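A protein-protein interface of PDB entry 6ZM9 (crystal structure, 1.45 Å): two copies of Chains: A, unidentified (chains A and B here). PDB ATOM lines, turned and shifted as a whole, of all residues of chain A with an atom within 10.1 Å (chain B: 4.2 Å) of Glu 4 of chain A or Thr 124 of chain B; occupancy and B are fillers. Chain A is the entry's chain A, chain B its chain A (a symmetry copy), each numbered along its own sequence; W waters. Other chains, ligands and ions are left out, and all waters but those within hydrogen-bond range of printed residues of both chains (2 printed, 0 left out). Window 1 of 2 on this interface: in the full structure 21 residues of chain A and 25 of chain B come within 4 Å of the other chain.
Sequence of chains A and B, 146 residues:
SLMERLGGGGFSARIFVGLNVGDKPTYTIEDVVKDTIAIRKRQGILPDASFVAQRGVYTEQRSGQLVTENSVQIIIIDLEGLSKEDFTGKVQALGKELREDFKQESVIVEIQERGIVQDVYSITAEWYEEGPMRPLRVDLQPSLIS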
ATOM      1  N   SER A   1      19.630 -17.276   0.110  1.00  0.00           N
ATOM      2  CA  SER A   1      18.362 -17.778   0.709  1.00  0.00           C
ATOM      3  C   SER A   1      17.203 -17.124  -0.020  1.00  0.00           C
ATOM      4  O   SER A   1      17.362 -16.066  -0.642  1.00  0.00           O
ATOM      5  CB  SER A   1      18.330 -17.477   2.203  1.00  0.00           C
ATOM      6  OG  SER A   1      18.480 -16.090   2.441  1.00  0.00           O
ATOM      7  N   LEU A   2      16.048 -17.782   0.037  1.00  0.00           N
ATOM      8  CA  LEU A   2      14.834 -17.274  -0.568  1.00  0.00           C
ATOM      9  C   LEU A   2      14.026 -16.528   0.483  1.00  0.00           C
ATOM     10  O   LEU A   2      13.852 -16.997   1.608  1.00  0.00           O
ATOM     11  CB  LEU A   2      13.982 -18.426  -1.086  1.00  0.00           C
ATOM     12  CG  LEU A   2      14.416 -19.111  -2.373  1.00  0.00           C
ATOM     13  CD1 LEU A   2      13.215 -19.906  -2.850  1.00  0.00           C
ATOM     14  CD2 LEU A   2      14.862 -18.140  -3.423  1.00  0.00           C
ATOM     15  N   MET A   3      13.520 -15.366   0.106  1.00  0.00           N
ATOM     16  CA  MET A   3      12.681 -14.549   0.979  1.00  0.00           C
ATOM     17  C   MET A   3      11.256 -14.775   0.487  1.00  0.00           C
ATOM     18  O   MET A   3      10.778 -14.076  -0.400  1.00  0.00           O
ATOM     19  CB  MET A   3      13.121 -13.097   0.838  1.00  0.00           C
ATOM     20  CG  MET A   3      12.277 -12.067   1.540  1.00  0.00           C
ATOM     21  SD  MET A   3      12.778 -11.789   3.246  1.00  0.00           S
ATOM     22  CE  MET A   3      14.580 -11.744   3.200  1.00  0.00           C
ATOM     23  N   GLU A   4      10.616 -15.775   1.038  1.00  0.00           N
ATOM     24  CA  GLU A   4       9.284 -16.120   0.535  1.00  0.00           C
ATOM     25  C   GLU A   4       8.195 -15.486   1.383  1.00  0.00           C
ATOM     26  O   GLU A   4       8.146 -15.680   2.603  1.00  0.00           O
ATOM     27  CB  GLU A   4       9.027 -17.621   0.343  1.00  0.00           C
ATOM     28  CG  GLU A   4       9.466 -18.520   1.445  1.00  0.00           C
ATOM     29  CD  GLU A   4      10.632 -19.400   1.021  1.00  0.00           C
ATOM     30  OE1 GLU A   4      10.379 -20.538   0.563  1.00  0.00           O
ATOM     31  OE2 GLU A   4      11.793 -18.944   1.122  1.00  0.00           O
ATOM     32  N   ARG A   5       7.323 -14.739   0.723  1.00  0.00           N
ATOM     33  CA  ARG A   5       6.232 -14.040   1.393  1.00  0.00           C
ATOM     34  C   ARG A   5       5.092 -15.008   1.617  1.00  0.00           C
ATOM     35  O   ARG A   5       4.701 -15.749   0.706  1.00  0.00           O
ATOM     36  CB  ARG A   5       5.719 -12.892   0.529  1.00  0.00           C
ATOM     37  CG  ARG A   5       6.473 -11.599   0.711  1.00  0.00           C
ATOM     38  CD  ARG A   5       5.901 -10.461  -0.143  1.00  0.00           C
ATOM     39  NE  ARG A   5       6.608  -9.212   0.144  1.00  0.00           N
ATOM     40  CZ  ARG A   5       7.843  -8.922  -0.269  1.00  0.00           C
ATOM     41  NH1 ARG A   5       8.533  -9.777  -1.019  1.00  0.00           N
ATOM     42  NH2 ARG A   5       8.391  -7.762   0.076  1.00  0.00           N
ATOM     43  N   LEU A   6       4.510 -15.008   2.783  1.00  0.00           N
ATOM     44  CA  LEU A   6       3.556 -16.018   3.095  1.00  0.00           C
ATOM     45  C   LEU A   6       2.206 -15.814   2.512  1.00  0.00           C
ATOM     46  O   LEU A   6       1.650 -14.707   2.564  1.00  0.00           O
ATOM     47  CB  LEU A   6       3.429 -16.145   4.615  1.00  0.00           C
ATOM     48  CG  LEU A   6       2.386 -17.144   5.125  1.00  0.00           C
ATOM     49  CD1 LEU A   6       2.741 -18.557   4.692  1.00  0.00           C
ATOM     50  CD2 LEU A   6       2.256 -17.059   6.639  1.00  0.00           C
ATOM     51  N   GLY A   7       1.591 -16.920   2.057  1.00  0.00           N
ATOM     52  CA  GLY A   7       0.320 -16.939   1.409  1.00  0.00           C
ATOM     53  C   GLY A   7      -0.838 -17.092   2.361  1.00  0.00           C
ATOM     54  O   GLY A   7      -0.701 -17.508   3.513  1.00  0.00           O
ATOM     55  N   LEU A  79       0.852 -21.397   8.271  1.00  0.00           N
ATOM     56  CA  LEU A  79       1.706 -21.492   7.095  1.00  0.00           C
ATOM     57  C   LEU A  79       1.065 -22.272   5.951  1.00  0.00           C
ATOM     58  O   LEU A  79       1.715 -22.461   4.919  1.00  0.00           O
ATOM     59  CB  LEU A  79       3.054 -22.156   7.459  1.00  0.00           C
ATOM     60  CG  LEU A  79       3.849 -21.502   8.585  1.00  0.00           C
ATOM     61  CD1 LEU A  79       5.206 -22.130   8.859  1.00  0.00           C
ATOM     62  CD2 LEU A  79       4.083 -20.032   8.304  1.00  0.00           C
ATOM     63  N   GLN B  61      11.334 -29.286   5.750  1.00  0.00           N
ATOM     64  CA  GLN B  61      10.645 -29.224   4.470  1.00  0.00           C
ATOM     65  C   GLN B  61      11.038 -30.362   3.539  1.00  0.00           C
ATOM     66  O   GLN B  61      10.196 -30.857   2.781  1.00  0.00           O
ATOM     67  CB  GLN B  61      10.905 -27.868   3.820  1.00  0.00           C
ATOM     68  CG  GLN B  61      10.438 -26.705   4.675  1.00  0.00           C
ATOM     69  CD  GLN B  61      10.994 -25.379   4.202  1.00  0.00           C
ATOM     70  OE1 GLN B  61      12.014 -25.333   3.506  1.00  0.00           O
ATOM     71  NE2 GLN B  61      10.331 -24.287   4.580  1.00  0.00           N
ATOM     72  N   GLU B 105      17.523 -24.000   8.498  1.00  0.00           N
ATOM     73  CA  GLU B 105      16.761 -24.231   7.278  1.00  0.00           C
ATOM     74  C   GLU B 105      15.832 -23.063   6.983  1.00  0.00           C
ATOM     75  O   GLU B 105      15.657 -22.677   5.820  1.00  0.00           O
ATOM     76  CB  GLU B 105      15.941 -25.518   7.350  1.00  0.00           C
ATOM     77  CG  GLU B 105      15.316 -25.835   5.999  1.00  0.00           C
ATOM     78  CD  GLU B 105      14.447 -27.068   5.996  1.00  0.00           C
ATOM     79  OE1 GLU B 105      13.481 -27.145   6.780  1.00  0.00           O
ATOM     80  OE2 GLU B 105      14.728 -27.955   5.174  1.00  0.00           O
ATOM     81  N   VAL B 120       4.687 -11.410   6.292  1.00  0.00           N
ATOM     82  CA  VAL B 120       5.316 -12.525   6.984  1.00  0.00           C
ATOM     83  C   VAL B 120       6.172 -13.223   5.942  1.00  0.00           C
ATOM     84  O   VAL B 120       5.682 -13.540   4.851  1.00  0.00           O
ATOM     85  CB  VAL B 120       4.306 -13.525   7.562  1.00  0.00           C
ATOM     86  CG1 VAL B 120       5.029 -14.670   8.249  1.00  0.00           C
ATOM     87  CG2 VAL B 120       3.413 -12.869   8.540  1.00  0.00           C
ATOM     88  N   TYR B 121       7.440 -13.424   6.263  1.00  0.00           N
ATOM     89  CA  TYR B 121       8.394 -14.031   5.363  1.00  0.00           C
ATOM     90  C   TYR B 121       8.948 -15.283   6.007  1.00  0.00           C
ATOM     91  O   TYR B 121       9.223 -15.300   7.212  1.00  0.00           O
ATOM     92  CB  TYR B 121       9.628 -13.110   5.112  1.00  0.00           C
ATOM     93  CG  TYR B 121       9.302 -11.735   4.626  1.00  0.00           C
ATOM     94  CD1 TYR B 121       9.060 -11.500   3.286  1.00  0.00           C
ATOM     95  CD2 TYR B 121       9.250 -10.668   5.504  1.00  0.00           C
ATOM     96  CE1 TYR B 121       8.752 -10.232   2.822  1.00  0.00           C
ATOM     97  CE2 TYR B 121       8.935  -9.396   5.055  1.00  0.00           C
ATOM     98  CZ  TYR B 121       8.690  -9.177   3.711  1.00  0.00           C
ATOM     99  OH  TYR B 121       8.382  -7.917   3.244  1.00  0.00           O
ATOM    100  N   SER B 122       9.130 -16.327   5.205  1.00  0.00           N
ATOM    101  CA  SER B 122       9.992 -17.457   5.575  1.00  0.00           C
ATOM    102  C   SER B 122      11.287 -17.312   4.789  1.00  0.00           C
ATOM    103  O   SER B 122      11.245 -17.282   3.557  1.00  0.00           O
ATOM    104  CB  SER B 122       9.297 -18.814   5.299  1.00  0.00           C
ATOM    105  OG  SER B 122      10.041 -19.876   5.899  1.00  0.00           O
ATOM    106  N   ILE B 123      12.395 -17.178   5.494  1.00  0.00           N
ATOM    107  CA  ILE B 123      13.691 -17.031   4.864  1.00  0.00           C
ATOM    108  C   ILE B 123      14.273 -18.423   4.828  1.00  0.00           C
ATOM    109  O   ILE B 123      14.601 -18.982   5.881  1.00  0.00           O
ATOM    110  CB  ILE B 123      14.600 -16.068   5.631  1.00  0.00           C
ATOM    111  CG1 ILE B 123      13.990 -14.684   5.672  1.00  0.00           C
ATOM    112  CG2 ILE B 123      15.974 -16.055   4.961  1.00  0.00           C
ATOM    113  CD1 ILE B 123      14.720 -13.712   6.590  1.00  0.00           C
ATOM    114  N   THR B 124      14.369 -19.007   3.638  1.00  0.00           N
ATOM    115  CA  THR B 124      14.601 -20.434   3.499  1.00  0.00           C
ATOM    116  C   THR B 124      15.929 -20.688   2.821  1.00  0.00           C
ATOM    117  O   THR B 124      16.240 -20.077   1.791  1.00  0.00           O
ATOM    118  CB  THR B 124      13.459 -21.068   2.709  1.00  0.00           C
ATOM    119  OG1 THR B 124      12.236 -20.809   3.404  1.00  0.00           O
ATOM    120  CG2 THR B 124      13.654 -22.549   2.597  1.00  0.00           C
ATOM    121  N   ALA B 125      16.688 -21.613   3.388  1.00  0.00           N
ATOM    122  CA  ALA B 125      17.967 -21.989   2.821  1.00  0.00           C
ATOM    123  C   ALA B 125      17.784 -22.616   1.446  1.00  0.00           C
ATOM    124  O   ALA B 125      16.846 -23.381   1.208  1.00  0.00           O
ATOM    125  CB  ALA B 125      18.630 -23.010   3.743  1.00  0.00           C
ATOM    126  N   GLU B 126      18.718 -22.321   0.547  1.00  0.00           N
ATOM    127  CA  GLU B 126      18.705 -22.851  -0.809  1.00  0.00           C
ATOM    128  C   GLU B 126      19.713 -23.983  -0.998  1.00  0.00           C
ATOM    129  O   GLU B 126      20.229 -24.187  -2.102  1.00  0.00           O
ATOM    130  CB  GLU B 126      18.933 -21.721  -1.807  1.00  0.00           C
ATOM    131  CG  GLU B 126      17.789 -20.717  -1.887  1.00  0.00           C
ATOM    132  CD  GLU B 126      18.105 -19.570  -2.836  1.00  0.00           C
ATOM    133  OE1 GLU B 126      18.261 -19.807  -4.041  1.00  0.00           O
ATOM    134  OE2 GLU B 126      18.259 -18.422  -2.396  1.00  0.00           O
HETATM  135  O   HOH W   1      10.166  -6.012   1.200  1.00  0.00           O
HETATM  136  O   HOH W   2       2.612 -12.356   4.299  1.00  0.00           O
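O of Thr 124 of chain B lies within hydrogen-bond range of N of Leu 2 of chain A (2.9 Å).
The backbone NH (N) of Leu 2 of chain A lies within hydrogen-bond range of the side-chain carboxylate (OE2) of Glu 126 of chain B (3.3 Å).
N of Ser 1 of chain A sits close to OE2 of Glu 126 of chain B (3.1 Å).
N of Leu 6 of chain A sits at hydrogen-bond distance from O of Val 120 of chain B (2.8 Å).
OG1 of Thr 124 of chain B sits at hydrogen-bond distance from OE2 of Glu 4 of chain A.
N of Ser 122 of chain B is in hydrogen-bond range of O of Glu 4 of chain A (2.9 Å).
The backbone carbonyl oxygen (O) of Leu 2 of chain A lies close to the backbone carbonyl oxygen (O) of Ser 122 of chain B, at 3.3 Å.
OH of Tyr 121 of chain B lies within hydrogen-bond range of NH2 of Arg 5 of chain A, at 3.2 Å.
The side-chain hydroxyl (OG) of Ser 122 of chain B lies within hydrogen-bond range of the side-chain hydroxyl (OG1) of Thr 124 of chain B, 3.5 Å away.
Among the printed residues, pairs that only touch across the chains: Ser 1 of chain A with Ile 123 of chain B (3.6 Å), Ser 1 of chain A with Thr 124 of chain B (3.3 Å), Leu 2 of chain A with Ile 123 of chain B (3.3 Å), Met 3 of chain A with Tyr 121 of chain B (3.7 Å), Met 3 of chain A with Ser 122 of chain B (3.96 Å), Met 3 of chain A with Ile 123 of chain B (3.9 Å), Glu 4 of chain A with Val 120 of chain B (3.96 Å), Glu 4 of chain A with Tyr 121 of chain B (3.2 Å) and Arg 5 of chain A with Val 120 of chain B (3.5 Å).
Of the printed residues of chain B, Glu 4 of chain A touches Val 120 (3.96 Å), Tyr 121 (3.2 Å), Ser 122 (2.9 Å) and Thr 124 (3.0 Å).
Of the printed residues of chain A, Thr 124 of chain B touches Ser 1, Leu 2 and Glu 4.
No residue of chain A comes within 4 Å of Ala 125 of chain B.
Of the printed residues of chain A, Val 120 of chain B touches Glu 4, Arg 5 and Leu 6.
Of the printed residues of chain B, Ser 1 of chain A touches Ile 123 (3.6 Å), Thr 124 (3.3 Å) and Glu 126 (2.9 Å).
Printed residues of chain B within 4 Å of Arg 5 of chain A: Val 120 and Tyr 121.
Printed residues of chain A within 4 Å of Ser 122 of chain B: Leu 2, Met 3 and Glu 4.
Of the printed residues of chain A, Glu 126 of chain B touches Ser 1 (2.9 Å) and Leu 2 (3.3 Å).
Leu 79 of chain A touches none of the printed residues of chain B.
Gly 7 of chain A touches none of the printed residues of chain B.
The nearest printed residue of chain B that does not touch Met 3 of chain A is Thr 124 of chain B (5.1 Å).
Of the 8 printed residues of chain A, 6 touch a printed residue of chain B.
Printed residues of chain A that touch a printed residue of chain B: Ser 1, Leu 2, Met 3, Glu 4, Arg 5 and Leu 6.
Along chain A the printed residues that touch a printed residue of chain B span positions 1 to 6.
Hydrophobic or aromatic side chains of chain B within 4 Å of the printed part of chain A: Val 120, Tyr 121 and Ile 123.
No position is printed for both chains.
Water W1 bridges the guanidinium group (NH2) of Arg 5 of chain A and the side-chain hydroxyl (OH) of Tyr 121 of chain B.
Water W2 lies within hydrogen-bond range of N of Val 120 of chain B and O of Leu 6 of chain A.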
